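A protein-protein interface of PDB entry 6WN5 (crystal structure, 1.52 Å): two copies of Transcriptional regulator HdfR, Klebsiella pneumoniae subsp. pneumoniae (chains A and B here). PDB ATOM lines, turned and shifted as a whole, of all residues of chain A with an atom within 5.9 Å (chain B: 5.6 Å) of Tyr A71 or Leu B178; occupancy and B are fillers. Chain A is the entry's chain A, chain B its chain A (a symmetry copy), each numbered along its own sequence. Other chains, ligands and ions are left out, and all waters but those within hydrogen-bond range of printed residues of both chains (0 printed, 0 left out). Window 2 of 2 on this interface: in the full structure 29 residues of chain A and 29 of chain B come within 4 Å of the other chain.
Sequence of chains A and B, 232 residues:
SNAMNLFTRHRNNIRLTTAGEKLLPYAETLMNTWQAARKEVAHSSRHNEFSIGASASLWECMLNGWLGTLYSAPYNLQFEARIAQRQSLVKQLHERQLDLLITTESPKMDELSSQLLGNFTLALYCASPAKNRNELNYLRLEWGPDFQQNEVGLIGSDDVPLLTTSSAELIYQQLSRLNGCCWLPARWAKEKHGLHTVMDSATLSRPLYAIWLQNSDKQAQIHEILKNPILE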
ATOM      1  N   LEU A  67     -30.423 -10.559 -14.285  1.00  0.00           N
ATOM      2  CA  LEU A  67     -30.141 -11.260 -15.556  1.00  0.00           C
ATOM      3  C   LEU A  67     -29.041 -12.302 -15.322  1.00  0.00           C
ATOM      4  O   LEU A  67     -29.146 -13.403 -15.875  1.00  0.00           O
ATOM      5  CB  LEU A  67     -29.692 -10.215 -16.582  1.00  0.00           C
ATOM      6  CG  LEU A  67     -29.137 -10.796 -17.880  1.00  0.00           C
ATOM      7  CD1 LEU A  67     -30.209 -11.560 -18.627  1.00  0.00           C
ATOM      8  CD2 LEU A  67     -28.544  -9.687 -18.733  1.00  0.00           C
ATOM      9  N   GLY A  68     -27.988 -11.960 -14.583  1.00  0.00           N
ATOM     10  CA  GLY A  68     -26.917 -12.920 -14.262  1.00  0.00           C
ATOM     11  C   GLY A  68     -27.440 -14.208 -13.663  1.00  0.00           C
ATOM     12  O   GLY A  68     -26.901 -15.297 -14.016  1.00  0.00           O
ATOM     13  N   THR A  69     -28.491 -14.135 -12.843  1.00  0.00           N
ATOM     14  CA  THR A  69     -29.037 -15.351 -12.188  1.00  0.00           C
ATOM     15  C   THR A  69     -29.829 -16.229 -13.169  1.00  0.00           C
ATOM     16  O   THR A  69     -30.045 -17.424 -12.852  1.00  0.00           O
ATOM     17  CB  THR A  69     -29.919 -14.994 -10.981  1.00  0.00           C
ATOM     18  OG1 THR A  69     -31.165 -14.418 -11.391  1.00  0.00           O
ATOM     19  CG2 THR A  69     -29.214 -14.059 -10.029  1.00  0.00           C
ATOM     20  N   LEU A  70     -30.242 -15.687 -14.314  1.00  0.00           N
ATOM     21  CA  LEU A  70     -31.117 -16.439 -15.245  1.00  0.00           C
ATOM     22  C   LEU A  70     -30.305 -17.486 -16.006  1.00  0.00           C
ATOM     23  O   LEU A  70     -30.902 -18.453 -16.489  1.00  0.00           O
ATOM     24  CB  LEU A  70     -31.787 -15.462 -16.211  1.00  0.00           C
ATOM     25  CG  LEU A  70     -32.703 -14.405 -15.580  1.00  0.00           C
ATOM     26  CD1 LEU A  70     -33.351 -13.557 -16.665  1.00  0.00           C
ATOM     27  CD2 LEU A  70     -33.760 -15.028 -14.685  1.00  0.00           C
ATOM     28  N   TYR A  71     -28.992 -17.308 -16.091  1.00  0.00           N
ATOM     29  CA  TYR A  71     -28.150 -18.246 -16.874  1.00  0.00           C
ATOM     30  C   TYR A  71     -27.959 -19.578 -16.134  1.00  0.00           C
ATOM     31  O   TYR A  71     -27.625 -20.520 -16.821  1.00  0.00           O
ATOM     32  CB  TYR A  71     -26.826 -17.593 -17.285  1.00  0.00           C
ATOM     33  CG  TYR A  71     -26.980 -16.543 -18.354  1.00  0.00           C
ATOM     34  CD1 TYR A  71     -27.026 -16.885 -19.695  1.00  0.00           C
ATOM     35  CD2 TYR A  71     -27.062 -15.202 -18.040  1.00  0.00           C
ATOM     36  CE1 TYR A  71     -27.216 -15.931 -20.684  1.00  0.00           C
ATOM     37  CE2 TYR A  71     -27.188 -14.223 -19.017  1.00  0.00           C
ATOM     38  CZ  TYR A  71     -27.259 -14.589 -20.353  1.00  0.00           C
ATOM     39  OH  TYR A  71     -27.402 -13.639 -21.329  1.00  0.00           O
ATOM     40  N   SER A  72     -28.189 -19.637 -14.814  1.00  0.00           N
ATOM     41  CA  SER A  72     -28.097 -20.902 -14.016  1.00  0.00           C
ATOM     42  C   SER A  72     -29.501 -21.390 -13.620  1.00  0.00           C
ATOM     43  O   SER A  72     -29.618 -22.231 -12.657  1.00  0.00           O
ATOM     44  CB  SER A  72     -27.332 -20.686 -12.786  1.00  0.00           C
ATOM     45  OG  SER A  72     -28.128 -19.951 -11.877  1.00  0.00           O
ATOM     46  N   ALA A  73     -30.533 -20.791 -14.211  1.00  0.00           N
ATOM     47  CA  ALA A  73     -31.923 -21.233 -13.944  1.00  0.00           C
ATOM     48  C   ALA A  73     -32.131 -22.551 -14.666  1.00  0.00           C
ATOM     49  O   ALA A  73     -31.495 -22.767 -15.701  1.00  0.00           O
ATOM     50  CB  ALA A  73     -32.909 -20.204 -14.411  1.00  0.00           C
ATOM     51  N   TYR A  75     -33.240 -23.918 -17.075  1.00  0.00           N
ATOM     52  CA  TYR A  75     -33.614 -23.883 -18.511  1.00  0.00           C
ATOM     53  C   TYR A  75     -32.437 -23.304 -19.294  1.00  0.00           C
ATOM     54  O   TYR A  75     -31.545 -22.680 -18.657  1.00  0.00           O
ATOM     55  CB  TYR A  75     -34.896 -23.080 -18.754  1.00  0.00           C
ATOM     56  CG  TYR A  75     -35.028 -21.804 -17.960  1.00  0.00           C
ATOM     57  CD1 TYR A  75     -34.526 -20.602 -18.435  1.00  0.00           C
ATOM     58  CD2 TYR A  75     -35.699 -21.792 -16.745  1.00  0.00           C
ATOM     59  CE1 TYR A  75     -34.633 -19.434 -17.698  1.00  0.00           C
ATOM     60  CE2 TYR A  75     -35.832 -20.629 -16.005  1.00  0.00           C
ATOM     61  CZ  TYR A  75     -35.299 -19.446 -16.485  1.00  0.00           C
ATOM     62  OH  TYR A  75     -35.399 -18.303 -15.752  1.00  0.00           O
ATOM     63  N   LEU A  77     -31.567 -20.698 -22.223  1.00  0.00           N
ATOM     64  CA  LEU A  77     -32.007 -19.575 -23.104  1.00  0.00           C
ATOM     65  C   LEU A  77     -30.833 -18.647 -23.427  1.00  0.00           C
ATOM     66  O   LEU A  77     -29.867 -18.604 -22.630  1.00  0.00           O
ATOM     67  CB  LEU A  77     -33.073 -18.718 -22.412  1.00  0.00           C
ATOM     68  CG  LEU A  77     -34.458 -19.325 -22.242  1.00  0.00           C
ATOM     69  CD1 LEU A  77     -35.356 -18.368 -21.464  1.00  0.00           C
ATOM     70  CD2 LEU A  77     -35.077 -19.681 -23.585  1.00  0.00           C
ATOM     71  N   GLN A  78     -30.964 -17.921 -24.543  1.00  0.00           N
ATOM     72  CA  GLN A  78     -30.057 -16.802 -24.881  1.00  0.00           C
ATOM     73  C   GLN A  78     -30.875 -15.528 -24.684  1.00  0.00           C
ATOM     74  O   GLN A  78     -32.079 -15.566 -24.878  1.00  0.00           O
ATOM     75  CB  GLN A  78     -29.501 -16.913 -26.290  1.00  0.00           C
ATOM     76  CG  GLN A  78     -28.719 -18.205 -26.528  1.00  0.00           C
ATOM     77  CD  GLN A  78     -29.628 -19.356 -26.859  1.00  0.00           C
ATOM     78  OE1 GLN A  78     -30.535 -19.221 -27.677  1.00  0.00           O
ATOM     79  NE2 GLN A  78     -29.386 -20.502 -26.231  1.00  0.00           N
ATOM     80  N   PHE A  79     -30.248 -14.452 -24.249  1.00  0.00           N
ATOM     81  CA  PHE A  79     -31.032 -13.251 -23.874  1.00  0.00           C
ATOM     82  C   PHE A  79     -30.594 -11.996 -24.615  1.00  0.00           C
ATOM     83  O   PHE A  79     -29.427 -11.862 -25.001  1.00  0.00           O
ATOM     84  CB  PHE A  79     -30.862 -12.954 -22.381  1.00  0.00           C
ATOM     85  CG  PHE A  79     -31.567 -13.941 -21.487  1.00  0.00           C
ATOM     86  CD1 PHE A  79     -32.921 -13.821 -21.245  1.00  0.00           C
ATOM     87  CD2 PHE A  79     -30.870 -14.974 -20.881  1.00  0.00           C
ATOM     88  CE1 PHE A  79     -33.581 -14.736 -20.439  1.00  0.00           C
ATOM     89  CE2 PHE A  79     -31.535 -15.903 -20.088  1.00  0.00           C
ATOM     90  CZ  PHE A  79     -32.872 -15.747 -19.832  1.00  0.00           C
ATOM     91  N   ASN B 137     -17.681 -17.995 -25.663  1.00  0.00           N
ATOM     92  CA  ASN B 137     -19.028 -17.624 -26.136  1.00  0.00           C
ATOM     93  C   ASN B 137     -18.985 -16.196 -26.665  1.00  0.00           C
ATOM     94  O   ASN B 137     -18.696 -15.265 -25.898  1.00  0.00           O
ATOM     95  CB  ASN B 137     -20.049 -17.722 -25.015  1.00  0.00           C
ATOM     96  CG  ASN B 137     -20.205 -19.141 -24.513  1.00  0.00           C
ATOM     97  OD1 ASN B 137     -20.327 -20.071 -25.307  1.00  0.00           O
ATOM     98  ND2 ASN B 137     -20.212 -19.311 -23.202  1.00  0.00           N
ATOM     99  N   LEU B 139     -20.338 -12.784 -27.468  1.00  0.00           N
ATOM    100  CA  LEU B 139     -21.463 -11.953 -27.006  1.00  0.00           C
ATOM    101  C   LEU B 139     -21.565 -10.764 -27.953  1.00  0.00           C
ATOM    102  O   LEU B 139     -20.526 -10.356 -28.496  1.00  0.00           O
ATOM    103  CB  LEU B 139     -21.240 -11.491 -25.566  1.00  0.00           C
ATOM    104  CG  LEU B 139     -20.845 -12.571 -24.540  1.00  0.00           C
ATOM    105  CD1 LEU B 139     -20.674 -11.958 -23.152  1.00  0.00           C
ATOM    106  CD2 LEU B 139     -21.853 -13.725 -24.517  1.00  0.00           C
ATOM    107  N   LEU B 162     -25.141 -15.715 -26.491  1.00  0.00           N
ATOM    108  CA  LEU B 162     -25.726 -15.924 -25.140  1.00  0.00           C
ATOM    109  C   LEU B 162     -26.299 -14.613 -24.604  1.00  0.00           C
ATOM    110  O   LEU B 162     -27.192 -14.668 -23.731  1.00  0.00           O
ATOM    111  CB  LEU B 162     -24.657 -16.444 -24.184  1.00  0.00           C
ATOM    112  CG  LEU B 162     -24.748 -17.910 -23.808  1.00  0.00           C
ATOM    113  CD1 LEU B 162     -24.716 -18.795 -25.047  1.00  0.00           C
ATOM    114  CD2 LEU B 162     -23.638 -18.255 -22.824  1.00  0.00           C
ATOM    115  N   LEU B 163     -25.670 -13.506 -24.994  1.00  0.00           N
ATOM    116  CA  LEU B 163     -26.134 -12.166 -24.598  1.00  0.00           C
ATOM    117  C   LEU B 163     -25.953 -11.211 -25.757  1.00  0.00           C
ATOM    118  O   LEU B 163     -24.883 -11.222 -26.385  1.00  0.00           O
ATOM    119  CB  LEU B 163     -25.365 -11.687 -23.375  1.00  0.00           C
ATOM    120  CG  LEU B 163     -25.712 -10.287 -22.881  1.00  0.00           C
ATOM    121  CD1 LEU B 163     -27.187 -10.176 -22.504  1.00  0.00           C
ATOM    122  CD2 LEU B 163     -24.830  -9.935 -21.700  1.00  0.00           C
ATOM    123  N   GLN B 174     -21.092  -9.108 -17.499  1.00  0.00           N
ATOM    124  CA  GLN B 174     -21.622 -10.471 -17.837  1.00  0.00           C
ATOM    125  C   GLN B 174     -20.520 -11.356 -18.406  1.00  0.00           C
ATOM    126  O   GLN B 174     -20.571 -12.583 -18.213  1.00  0.00           O
ATOM    127  CB  GLN B 174     -22.814 -10.361 -18.793  1.00  0.00           C
ATOM    128  CG  GLN B 174     -24.009  -9.664 -18.157  1.00  0.00           C
ATOM    129  CD  GLN B 174     -24.738 -10.554 -17.187  1.00  0.00           C
ATOM    130  OE1 GLN B 174     -24.772 -11.771 -17.356  1.00  0.00           O
ATOM    131  NE2 GLN B 174     -25.306  -9.945 -16.156  1.00  0.00           N
ATOM    132  N   LEU B 175     -19.578 -10.785 -19.110  1.00  0.00           N
ATOM    133  CA  LEU B 175     -18.518 -11.511 -19.826  1.00  0.00           C
ATOM    134  C   LEU B 175     -17.744 -12.422 -18.855  1.00  0.00           C
ATOM    135  O   LEU B 175     -17.466 -13.593 -19.215  1.00  0.00           O
ATOM    136  CB  LEU B 175     -17.714 -10.375 -20.437  1.00  0.00           C
ATOM    137  CG  LEU B 175     -16.447 -10.677 -21.178  1.00  0.00           C
ATOM    138  CD1 LEU B 175     -15.987  -9.402 -21.874  1.00  0.00           C
ATOM    139  CD2 LEU B 175     -15.391 -11.181 -20.252  1.00  0.00           C
ATOM    140  N   SER B 176     -17.574 -11.985 -17.614  1.00  0.00           N
ATOM    141  CA  SER B 176     -16.775 -12.784 -16.658  1.00  0.00           C
ATOM    142  C   SER B 176     -17.549 -13.999 -16.171  1.00  0.00           C
ATOM    143  O   SER B 176     -16.934 -14.890 -15.586  1.00  0.00           O
ATOM    144  CB  SER B 176     -16.383 -11.952 -15.483  1.00  0.00           C
ATOM    145  OG  SER B 176     -17.530 -11.401 -14.861  1.00  0.00           O
ATOM    146  N   ARG B 177     -18.860 -14.049 -16.418  1.00  0.00           N
ATOM    147  CA  ARG B 177     -19.628 -15.224 -15.921  1.00  0.00           C
ATOM    148  C   ARG B 177     -20.238 -16.009 -17.087  1.00  0.00           C
ATOM    149  O   ARG B 177     -20.836 -17.076 -16.820  1.00  0.00           O
ATOM    150  CB  ARG B 177     -20.683 -14.775 -14.915  1.00  0.00           C
ATOM    151  CG  ARG B 177     -20.061 -14.313 -13.604  1.00  0.00           C
ATOM    152  CD  ARG B 177     -20.984 -13.488 -12.740  1.00  0.00           C
ATOM    153  NE  ARG B 177     -22.197 -14.171 -12.345  1.00  0.00           N
ATOM    154  CZ  ARG B 177     -23.368 -14.033 -12.944  1.00  0.00           C
ATOM    155  NH1 ARG B 177     -24.417 -14.671 -12.461  1.00  0.00           N
ATOM    156  NH2 ARG B 177     -23.485 -13.239 -13.998  1.00  0.00           N
ATOM    157  N   LEU B 178     -20.035 -15.545 -18.323  1.00  0.00           N
ATOM    158  CA  LEU B 178     -20.576 -16.246 -19.510  1.00  0.00           C
ATOM    159  C   LEU B 178     -19.449 -16.784 -20.383  1.00  0.00           C
ATOM    160  O   LEU B 178     -19.693 -17.053 -21.571  1.00  0.00           O
ATOM    161  CB  LEU B 178     -21.439 -15.277 -20.317  1.00  0.00           C
ATOM    162  CG  LEU B 178     -22.650 -14.715 -19.589  1.00  0.00           C
ATOM    163  CD1 LEU B 178     -23.459 -13.867 -20.571  1.00  0.00           C
ATOM    164  CD2 LEU B 178     -23.506 -15.800 -19.007  1.00  0.00           C
ATOM    165  N   ASN B 179     -18.263 -17.012 -19.823  1.00  0.00           N
ATOM    166  CA  ASN B 179     -17.109 -17.485 -20.653  1.00  0.00           C
ATOM    167  C   ASN B 179     -17.070 -16.688 -21.972  1.00  0.00           C
ATOM    168  O   ASN B 179     -16.910 -17.309 -23.037  1.00  0.00           O
ATOM    169  CB  ASN B 179     -17.195 -18.986 -20.926  1.00  0.00           C
ATOM    170  CG  ASN B 179     -15.899 -19.563 -21.484  1.00  0.00           C
ATOM    171  OD1 ASN B 179     -14.816 -19.169 -21.031  1.00  0.00           O
ATOM    172  ND2 ASN B 179     -16.000 -20.425 -22.483  1.00  0.00           N
ATOM    173  N   GLY B 180     -17.177 -15.368 -21.898  1.00  0.00           N
ATOM    174  CA  GLY B 180     -17.503 -14.613 -23.115  1.00  0.00           C
ATOM    175  C   GLY B 180     -16.374 -13.840 -23.721  1.00  0.00           C
ATOM    176  O   GLY B 180     -15.282 -13.633 -23.081  1.00  0.00           O
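No position is printed for both chains.
Of the 9 pairs that touch across the chains among the printed residues, none has its exchanged pair printed and touching as well.
The side-chain amide nitrogen (ND2) of Asn B137 sits at hydrogen-bond distance from the backbone carbonyl oxygen (O) of Leu B178.
Among the printed residues, merely in contact across the chains: Phe A79 with Leu B163 (3.3 Å), Tyr A71 with Leu B163 (3.5 Å), Tyr A71 with Leu B178 (3.6 Å), Gly A68 with Gln B174 (3.7 Å), Gln A78 with Leu B162 (3.8 Å) and Tyr A71 with Gln B174 (3.8 Å).
Of the printed residues of chain B, Tyr A71 touches Leu B162, Leu B163, Gln B174 and Leu B178.
Of the printed residues of chain A, Leu B178 touches Tyr A71.
Of the printed residues of chain A, Leu B162 touches Tyr A71, Gln A78 and Phe A79.
Of the printed residues of chain B, Gly A68 touches Gln B174 and Arg B177.
Printed residues of chain A within 4 Å of Leu B163: Tyr A71 and Phe A79.
Leu B139 touches none of the printed residues of chain A.
Ser A72 touches none of the printed residues of chain B.
The nearest printed residue of chain A that does not touch Leu B178 is Gly A68 (6.1 Å).
The nearest printed residue of chain B that does not touch Gly A68 is Leu B178 (6.1 Å).
O of Gly A68 lies within hydrogen-bond range of NH1 of Arg B177 (3.0 Å).
The backbone NH (N) of Phe A79 is in hydrogen-bond range of the backbone carbonyl oxygen (O) of Leu B162, 3.1 Å away.
The backbone carbonyl oxygen (O) of Leu B162 sits at hydrogen-bond distance from the side-chain hydroxyl (OH) of Tyr A71.
Of the 11 printed residues of chain A, 4 touch a printed residue of chain B.
Hydrophobic or aromatic side chains of chain A within 4 Å of the printed part of chain B: Tyr A71.
Of the 11 printed residues of chain B, 5 touch a printed residue of chain A.
Hydrophobic or aromatic side chains of chain B within 4 Å of the printed part of chain A: Leu B163 and Leu B178.
Among the printed residues, no Asp or Glu carboxylate lies within 4 Å of a Lys or Arg side-chain nitrogen of the other chain.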
